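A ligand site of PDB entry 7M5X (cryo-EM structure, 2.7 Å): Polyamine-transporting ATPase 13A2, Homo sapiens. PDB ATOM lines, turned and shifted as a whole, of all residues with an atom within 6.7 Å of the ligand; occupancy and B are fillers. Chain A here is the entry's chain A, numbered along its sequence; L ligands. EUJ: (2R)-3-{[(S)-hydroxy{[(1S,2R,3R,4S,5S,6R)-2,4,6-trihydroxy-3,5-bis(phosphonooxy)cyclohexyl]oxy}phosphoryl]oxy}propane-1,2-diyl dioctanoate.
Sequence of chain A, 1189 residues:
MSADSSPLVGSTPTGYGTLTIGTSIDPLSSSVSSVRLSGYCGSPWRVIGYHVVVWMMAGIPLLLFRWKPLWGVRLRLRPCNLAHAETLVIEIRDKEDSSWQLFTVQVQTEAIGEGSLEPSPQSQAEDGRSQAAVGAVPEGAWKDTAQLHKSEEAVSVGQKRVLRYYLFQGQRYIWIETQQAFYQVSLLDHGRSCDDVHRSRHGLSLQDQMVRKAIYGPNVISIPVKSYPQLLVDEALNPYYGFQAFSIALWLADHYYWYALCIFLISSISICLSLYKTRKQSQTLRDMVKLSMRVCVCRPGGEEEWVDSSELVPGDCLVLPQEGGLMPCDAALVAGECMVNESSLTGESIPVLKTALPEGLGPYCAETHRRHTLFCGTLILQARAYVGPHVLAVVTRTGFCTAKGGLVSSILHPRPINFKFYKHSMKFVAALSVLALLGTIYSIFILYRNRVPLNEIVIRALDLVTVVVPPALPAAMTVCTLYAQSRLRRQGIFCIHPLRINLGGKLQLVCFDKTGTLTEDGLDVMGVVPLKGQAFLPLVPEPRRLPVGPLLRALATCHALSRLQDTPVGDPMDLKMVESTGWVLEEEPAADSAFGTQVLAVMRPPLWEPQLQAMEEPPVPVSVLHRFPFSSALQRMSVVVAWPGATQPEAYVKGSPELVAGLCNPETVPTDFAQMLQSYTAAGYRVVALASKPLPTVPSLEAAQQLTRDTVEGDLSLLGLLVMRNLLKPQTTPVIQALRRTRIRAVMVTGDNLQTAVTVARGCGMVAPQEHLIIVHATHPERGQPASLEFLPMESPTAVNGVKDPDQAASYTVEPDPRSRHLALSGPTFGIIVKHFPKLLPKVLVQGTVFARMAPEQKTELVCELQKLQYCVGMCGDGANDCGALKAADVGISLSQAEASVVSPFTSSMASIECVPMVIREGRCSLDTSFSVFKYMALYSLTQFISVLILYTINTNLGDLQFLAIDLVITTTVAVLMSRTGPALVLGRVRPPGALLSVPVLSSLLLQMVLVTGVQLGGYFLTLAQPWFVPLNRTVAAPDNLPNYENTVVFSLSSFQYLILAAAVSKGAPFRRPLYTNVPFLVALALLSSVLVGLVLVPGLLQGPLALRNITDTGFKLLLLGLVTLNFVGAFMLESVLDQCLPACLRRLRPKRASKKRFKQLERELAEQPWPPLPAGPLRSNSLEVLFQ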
ATOM      1  N   PRO A 992      -4.380  14.254 -22.891  1.00  0.00           N
ATOM      2  CA  PRO A 992      -3.793  15.013 -23.984  1.00  0.00           C
ATOM      3  C   PRO A 992      -2.327  15.298 -23.710  1.00  0.00           C
ATOM      4  O   PRO A 992      -1.849  15.082 -22.591  1.00  0.00           O
ATOM      5  CB  PRO A 992      -4.623  16.303 -24.006  1.00  0.00           C
ATOM      6  CG  PRO A 992      -5.082  16.463 -22.628  1.00  0.00           C
ATOM      7  CD  PRO A 992      -5.300  15.073 -22.090  1.00  0.00           C
ATOM      8  N   PRO A 993      -1.575  15.758 -24.718  1.00  0.00           N
ATOM      9  CA  PRO A 993      -0.177  16.115 -24.464  1.00  0.00           C
ATOM     10  C   PRO A 993      -0.076  17.224 -23.420  1.00  0.00           C
ATOM     11  O   PRO A 993      -0.882  18.159 -23.406  1.00  0.00           O
ATOM     12  CB  PRO A 993       0.326  16.595 -25.832  1.00  0.00           C
ATOM     13  CG  PRO A 993      -0.606  15.986 -26.814  1.00  0.00           C
ATOM     14  CD  PRO A 993      -1.936  15.915 -26.131  1.00  0.00           C
ATOM     15  N   GLY A 994       0.923  17.108 -22.545  1.00  0.00           N
ATOM     16  CA  GLY A 994       1.086  18.038 -21.451  1.00  0.00           C
ATOM     17  C   GLY A 994       2.104  19.128 -21.721  1.00  0.00           C
ATOM     18  O   GLY A 994       1.854  20.304 -21.450  1.00  0.00           O
ATOM     19  N   ALA A 995       3.270  18.749 -22.257  1.00  0.00           N
ATOM     20  CA  ALA A 995       4.384  19.662 -22.464  1.00  0.00           C
ATOM     21  C   ALA A 995       4.299  20.248 -23.872  1.00  0.00           C
ATOM     22  O   ALA A 995       4.253  19.506 -24.847  1.00  0.00           O
ATOM     23  CB  ALA A 995       5.710  18.949 -22.259  1.00  0.00           C
ATOM     24  N   LEU A 996       4.300  21.588 -23.956  1.00  0.00           N
ATOM     25  CA  LEU A 996       4.271  22.243 -25.257  1.00  0.00           C
ATOM     26  C   LEU A 996       5.569  22.044 -26.025  1.00  0.00           C
ATOM     27  O   LEU A 996       5.560  22.133 -27.256  1.00  0.00           O
ATOM     28  CB  LEU A 996       3.987  23.732 -25.098  1.00  0.00           C
ATOM     29  CG  LEU A 996       2.530  24.142 -24.859  1.00  0.00           C
ATOM     30  CD1 LEU A 996       2.100  23.807 -23.437  1.00  0.00           C
ATOM     31  CD2 LEU A 996       2.331  25.624 -25.133  1.00  0.00           C
ATOM     32  N   LEU A 997       6.678  21.781 -25.334  1.00  0.00           N
ATOM     33  CA  LEU A 997       7.967  21.522 -25.955  1.00  0.00           C
ATOM     34  C   LEU A 997       8.163  20.058 -26.322  1.00  0.00           C
ATOM     35  O   LEU A 997       9.297  19.597 -26.455  1.00  0.00           O
ATOM     36  CB  LEU A 997       9.096  21.991 -25.030  1.00  0.00           C
ATOM     37  CG  LEU A 997      10.427  22.353 -25.689  1.00  0.00           C
ATOM     38  CD1 LEU A 997      10.357  23.710 -26.363  1.00  0.00           C
ATOM     39  CD2 LEU A 997      11.550  22.329 -24.656  1.00  0.00           C
ATOM     40  N   SER A 998       7.071  19.312 -26.472  1.00  0.00           N
ATOM     41  CA  SER A 998       7.144  17.895 -26.764  1.00  0.00           C
ATOM     42  C   SER A 998       7.649  17.664 -28.194  1.00  0.00           C
ATOM     43  O   SER A 998       7.607  18.558 -29.045  1.00  0.00           O
ATOM     44  CB  SER A 998       5.786  17.230 -26.592  1.00  0.00           C
ATOM     45  OG  SER A 998       4.858  17.713 -27.544  1.00  0.00           O
ATOM     46  N   VAL A 999       8.129  16.449 -28.427  1.00  0.00           N
ATOM     47  CA  VAL A 999       8.591  16.073 -29.771  1.00  0.00           C
ATOM     48  C   VAL A 999       7.497  16.264 -30.815  1.00  0.00           C
ATOM     49  O   VAL A 999       7.793  16.806 -31.887  1.00  0.00           O
ATOM     50  CB  VAL A 999       9.163  14.657 -29.754  1.00  0.00           C
ATOM     51  CG1 VAL A 999       9.429  14.175 -31.174  1.00  0.00           C
ATOM     52  CG2 VAL A 999      10.440  14.612 -28.931  1.00  0.00           C
ATOM     53  N   PRO A1000       6.263  15.797 -30.615  1.00  0.00           N
ATOM     54  CA  PRO A1000       5.237  16.020 -31.651  1.00  0.00           C
ATOM     55  C   PRO A1000       4.993  17.486 -31.977  1.00  0.00           C
ATOM     56  O   PRO A1000       4.879  17.831 -33.162  1.00  0.00           O
ATOM     57  CB  PRO A1000       3.980  15.360 -31.068  1.00  0.00           C
ATOM     58  CG  PRO A1000       4.300  15.078 -29.639  1.00  0.00           C
ATOM     59  CD  PRO A1000       5.768  14.861 -29.590  1.00  0.00           C
ATOM     60  N   LEU A1002       7.048  20.128 -31.648  1.00  0.00           N
ATOM     61  CA  LEU A1002       8.189  20.691 -32.365  1.00  0.00           C
ATOM     62  C   LEU A1002       8.285  20.120 -33.774  1.00  0.00           C
ATOM     63  O   LEU A1002       8.568  20.860 -34.715  1.00  0.00           O
ATOM     64  CB  LEU A1002       9.480  20.418 -31.592  1.00  0.00           C
ATOM     65  CG  LEU A1002       9.889  21.530 -30.626  1.00  0.00           C
ATOM     66  CD1 LEU A1002       8.840  21.728 -29.559  1.00  0.00           C
ATOM     67  CD2 LEU A1002      11.242  21.228 -30.010  1.00  0.00           C
ATOM     68  N   CYS A1145       7.099   5.703 -34.527  1.00  0.00           N
ATOM     69  CA  CYS A1145       8.527   6.029 -34.612  1.00  0.00           C
ATOM     70  C   CYS A1145       9.114   6.319 -33.240  1.00  0.00           C
ATOM     71  O   CYS A1145      10.237   5.900 -32.951  1.00  0.00           O
ATOM     72  CB  CYS A1145       8.731   7.213 -35.549  1.00  0.00           C
ATOM     73  SG  CYS A1145      10.467   7.589 -35.906  1.00  0.00           S
ATOM     74  N   LEU A1146       8.375   7.033 -32.387  1.00  0.00           N
ATOM     75  CA  LEU A1146       8.867   7.320 -31.048  1.00  0.00           C
ATOM     76  C   LEU A1146       9.077   6.038 -30.247  1.00  0.00           C
ATOM     77  O   LEU A1146      10.093   5.881 -29.557  1.00  0.00           O
ATOM     78  CB  LEU A1146       7.906   8.256 -30.313  1.00  0.00           C
ATOM     79  CG  LEU A1146       7.795   9.682 -30.859  1.00  0.00           C
ATOM     80  CD1 LEU A1146       6.666  10.422 -30.154  1.00  0.00           C
ATOM     81  CD2 LEU A1146       9.108  10.443 -30.716  1.00  0.00           C
ATOM     82  N   ARG A1147       8.116   5.110 -30.313  1.00  0.00           N
ATOM     83  CA  ARG A1147       8.259   3.858 -29.572  1.00  0.00           C
ATOM     84  C   ARG A1147       9.377   3.004 -30.141  1.00  0.00           C
ATOM     85  O   ARG A1147      10.145   2.395 -29.386  1.00  0.00           O
ATOM     86  CB  ARG A1147       6.932   3.097 -29.602  1.00  0.00           C
ATOM     87  CG  ARG A1147       5.803   3.800 -28.861  1.00  0.00           C
ATOM     88  CD  ARG A1147       4.520   3.005 -28.947  1.00  0.00           C
ATOM     89  NE  ARG A1147       4.621   1.730 -28.224  1.00  0.00           N
ATOM     90  CZ  ARG A1147       4.672   0.520 -28.774  1.00  0.00           C
ATOM     91  NH1 ARG A1147       4.652   0.344 -30.082  1.00  0.00           N
ATOM     92  NH2 ARG A1147       4.753  -0.544 -27.986  1.00  0.00           N
ATOM     93  N   LEU A1149      12.068   3.890 -31.375  1.00  0.00           N
ATOM     94  CA  LEU A1149      13.353   4.500 -31.057  1.00  0.00           C
ATOM     95  C   LEU A1149      13.458   4.660 -29.551  1.00  0.00           C
ATOM     96  O   LEU A1149      12.600   5.305 -28.934  1.00  0.00           O
ATOM     97  CB  LEU A1149      13.506   5.859 -31.751  1.00  0.00           C
ATOM     98  CG  LEU A1149      13.507   5.851 -33.277  1.00  0.00           C
ATOM     99  CD1 LEU A1149      13.456   7.278 -33.802  1.00  0.00           C
ATOM    100  CD2 LEU A1149      14.727   5.124 -33.819  1.00  0.00           C
ATOM    101  N   ARG A1150      14.496   4.080 -28.956  1.00  0.00           N
ATOM    102  CA  ARG A1150      14.692   4.140 -27.514  1.00  0.00           C
ATOM    103  C   ARG A1150      13.498   3.504 -26.819  1.00  0.00           C
ATOM    104  O   ARG A1150      12.772   4.192 -26.084  1.00  0.00           O
ATOM    105  CB  ARG A1150      14.861   5.593 -27.058  1.00  0.00           C
ATOM    106  N   ARG A1153      11.454   3.230 -22.230  1.00  0.00           N
ATOM    107  CA  ARG A1153      10.819   4.506 -21.909  1.00  0.00           C
ATOM    108  C   ARG A1153      11.060   4.881 -20.456  1.00  0.00           C
ATOM    109  O   ARG A1153      11.741   5.870 -20.173  1.00  0.00           O
ATOM    110  CB  ARG A1153       9.316   4.423 -22.211  1.00  0.00           C
ATOM    111  CG  ARG A1153       8.974   4.120 -23.674  1.00  0.00           C
ATOM    112  CD  ARG A1153       9.219   5.316 -24.573  1.00  0.00           C
ATOM    113  NE  ARG A1153       8.320   6.434 -24.275  1.00  0.00           N
ATOM    114  CZ  ARG A1153       8.362   7.618 -24.870  1.00  0.00           C
ATOM    115  NH1 ARG A1153       9.256   7.890 -25.802  1.00  0.00           N
ATOM    116  NH2 ARG A1153       7.485   8.551 -24.515  1.00  0.00           N
ATOM    117  N   ALA A1154      10.527   4.088 -19.523  1.00  0.00           N
ATOM    118  CA  ALA A1154      10.735   4.288 -18.093  1.00  0.00           C
ATOM    119  C   ALA A1154      10.402   5.720 -17.683  1.00  0.00           C
ATOM    120  O   ALA A1154      11.274   6.511 -17.319  1.00  0.00           O
ATOM    121  CB  ALA A1154      12.163   3.912 -17.692  1.00  0.00           C
ATOM    122  N   SER A1155       9.103   6.035 -17.784  1.00  0.00           N
ATOM    123  CA  SER A1155       8.617   7.409 -17.619  1.00  0.00           C
ATOM    124  C   SER A1155       9.174   8.056 -16.360  1.00  0.00           C
ATOM    125  O   SER A1155       9.261   7.428 -15.302  1.00  0.00           O
ATOM    126  CB  SER A1155       7.090   7.415 -17.578  1.00  0.00           C
ATOM    127  OG  SER A1155       6.586   8.722 -17.819  1.00  0.00           O
ATOM    128  N   LYS A1156       9.548   9.325 -16.492  1.00  0.00           N
ATOM    129  CA  LYS A1156      10.347  10.008 -15.487  1.00  0.00           C
ATOM    130  C   LYS A1156       9.538  10.498 -14.304  1.00  0.00           C
ATOM    131  O   LYS A1156      10.132  10.892 -13.295  1.00  0.00           O
ATOM    132  CB  LYS A1156      11.085  11.184 -16.115  1.00  0.00           C
ATOM    133  CG  LYS A1156      11.660  10.923 -17.516  1.00  0.00           C
ATOM    134  CD  LYS A1156      12.523   9.667 -17.562  1.00  0.00           C
ATOM    135  CE  LYS A1156      13.127   9.445 -18.946  1.00  0.00           C
ATOM    136  NZ  LYS A1156      12.090   9.407 -20.014  1.00  0.00           N
ATOM    137  N   LYS A1157       8.214  10.492 -14.389  1.00  0.00           N
ATOM    138  CA  LYS A1157       7.393  10.977 -13.286  1.00  0.00           C
ATOM    139  C   LYS A1157       7.599  10.112 -12.052  1.00  0.00           C
ATOM    140  O   LYS A1157       7.672   8.883 -12.136  1.00  0.00           O
ATOM    141  CB  LYS A1157       5.919  11.000 -13.686  1.00  0.00           C
ATOM    142  CG  LYS A1157       5.644  11.834 -14.928  1.00  0.00           C
ATOM    143  CD  LYS A1157       4.157  11.961 -15.205  1.00  0.00           C
ATOM    144  CE  LYS A1157       3.545  13.115 -14.438  1.00  0.00           C
ATOM    145  NZ  LYS A1157       3.961  14.433 -14.987  1.00  0.00           N
ATOM    146  N   LYS A1160       5.048   7.330 -11.223  1.00  0.00           N
ATOM    147  CA  LYS A1160       5.156   6.200 -12.136  1.00  0.00           C
ATOM    148  C   LYS A1160       6.367   5.335 -11.805  1.00  0.00           C
ATOM    149  O   LYS A1160       6.296   4.093 -11.866  1.00  0.00           O
ATOM    150  CB  LYS A1160       5.221   6.698 -13.574  1.00  0.00           C
ATOM    151  CG  LYS A1160       3.994   7.486 -14.021  1.00  0.00           C
ATOM    152  CD  LYS A1160       4.095   7.895 -15.486  1.00  0.00           C
ATOM    153  CE  LYS A1160       2.774   8.427 -16.004  1.00  0.00           C
ATOM    154  NZ  LYS A1160       2.856   8.837 -17.432  1.00  0.00           N
HETATM  155  C1  EUJ L   1       7.326  12.692 -22.394  1.00  0.00           C
HETATM  156  C2  EUJ L   1       6.465  11.443 -22.294  1.00  0.00           C
HETATM  157  C3  EUJ L   1       5.907  11.101 -20.918  1.00  0.00           C
HETATM  158  C4  EUJ L   1       5.240  12.278 -20.251  1.00  0.00           C
HETATM  159  C5  EUJ L   1       5.956  13.618 -20.447  1.00  0.00           C
HETATM  160  C6  EUJ L   1       7.323  13.500 -21.100  1.00  0.00           C
HETATM  161  O1  EUJ L   1       6.857  13.515 -23.543  1.00  0.00           O
HETATM  162  O2  EUJ L   1       5.355  11.622 -23.174  1.00  0.00           O
HETATM  163  O3  EUJ L   1       4.915  10.101 -21.330  1.00  0.00           O
HETATM  164  O4  EUJ L   1       3.913  12.349 -20.742  1.00  0.00           O
HETATM  165  O5  EUJ L   1       5.101  14.459 -21.294  1.00  0.00           O
HETATM  166  O6  EUJ L   1       8.207  12.874 -20.180  1.00  0.00           O
HETATM  167  P1  EUJ L   1       7.334  13.088 -24.999  1.00  0.00           P
HETATM  168  O11 EUJ L   1       7.296  14.296 -25.895  1.00  0.00           O
HETATM  169  O12 EUJ L   1       6.612  11.851 -25.472  1.00  0.00           O
HETATM  170  O13 EUJ L   1       8.880  12.690 -24.787  1.00  0.00           O
HETATM  171  P3  EUJ L   1       4.213   9.062 -20.395  1.00  0.00           P
HETATM  172  O31 EUJ L   1       4.546   9.943 -19.242  1.00  0.00           O
HETATM  173  O32 EUJ L   1       2.727   8.957 -20.663  1.00  0.00           O
HETATM  174  O33 EUJ L   1       4.935   7.722 -20.356  1.00  0.00           O
HETATM  175  P5  EUJ L   1       3.845  15.197 -20.590  1.00  0.00           P
HETATM  176  O51 EUJ L   1       2.632  14.823 -21.429  1.00  0.00           O
HETATM  177  O52 EUJ L   1       4.133  16.679 -20.614  1.00  0.00           O
HETATM  178  O53 EUJ L   1       3.738  14.662 -19.173  1.00  0.00           O
HETATM  179  C1A EUJ L   1      11.653   9.815 -26.859  1.00  0.00           C
HETATM  180  C1B EUJ L   1      12.105  14.960 -25.657  1.00  0.00           C
HETATM  181  C1C EUJ L   1       9.450  11.569 -25.529  1.00  0.00           C
HETATM  182  C2A EUJ L   1      12.976   9.493 -27.492  1.00  0.00           C
HETATM  183  C2B EUJ L   1      11.879  16.369 -25.193  1.00  0.00           C
HETATM  184  C2C EUJ L   1      10.920  11.809 -25.799  1.00  0.00           C
HETATM  185  C3A EUJ L   1      13.335  10.422 -28.629  1.00  0.00           C
HETATM  186  C3B EUJ L   1      11.488  17.301 -26.294  1.00  0.00           C
HETATM  187  C3C EUJ L   1      11.493  12.821 -24.840  1.00  0.00           C
HETATM  188  C4A EUJ L   1      13.914  11.761 -28.163  1.00  0.00           C
HETATM  189  C4B EUJ L   1      12.646  17.666 -27.204  1.00  0.00           C
HETATM  190  C5A EUJ L   1      14.802  12.477 -29.183  1.00  0.00           C
HETATM  191  C5B EUJ L   1      13.063  19.120 -27.125  1.00  0.00           C
HETATM  192  C6A EUJ L   1      15.710  13.504 -28.568  1.00  0.00           C
HETATM  193  C6B EUJ L   1      13.961  19.548 -28.251  1.00  0.00           C
HETATM  194  C7A EUJ L   1      16.308  14.464 -29.554  1.00  0.00           C
HETATM  195  C7B EUJ L   1      14.932  20.655 -27.900  1.00  0.00           C
HETATM  196  C8A EUJ L   1      16.400  15.859 -29.016  1.00  0.00           C
HETATM  197  C8B EUJ L   1      16.103  20.766 -28.845  1.00  0.00           C
HETATM  198  O1A EUJ L   1      10.661   9.592 -27.497  1.00  0.00           O
HETATM  199  O1B EUJ L   1      13.055  14.585 -26.308  1.00  0.00           O
HETATM  200  O2C EUJ L   1      11.622  10.534 -25.721  1.00  0.00           O
HETATM  201  O3C EUJ L   1      11.069  14.125 -25.290  1.00  0.00           O
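The backbone NH (N) of Ala 995 lies within hydrogen-bond range of an oxygen (O52) of the ligand, at 2.8 Å. The backbone NH (N) of Val 999 is in hydrogen-bond range of an oxygen (O11) of the ligand, 3.4 Å away. The backbone NH (N) of Gly 994 is in hydrogen-bond range of an oxygen (O51) of the ligand, at 3.1 Å. An oxygen (O12) of the ligand is in salt-bridge range of the guanidinium group (NH2) of Arg 1153 (3.5 Å). An oxygen (O31) of the ligand is in salt-bridge range of the side-chain amino group of Lys 1160 (2.7 Å). An oxygen (O31) of the ligand lies within hydrogen-bond range of the side-chain hydroxyl (OG) of Ser 1155.
OG of Ser 998 lies close to O of Ala 995 (3.3 Å).
Leu 997 touches the ligand. CB of Ser 998 touches O11 of the ligand (3.4 Å). Leu 1002 touches the ligand. CD2 of Leu 1146 touches O1A of the ligand, at 3.7 Å. Hydrophobic or aromatic side chains that line the ligand: Ala 995, Val 999, Leu 1002 and Leu 1146. Ten residues have an atom within 4 Å of the ligand: Gly 994, Ala 995, Leu 997, Ser 998, Val 999, Leu 1002, Leu 1146, Arg 1153, Ser 1155 and Lys 1160. The nearest printed residue that does not touch the ligand is Pro 1000 (4.04 Å).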
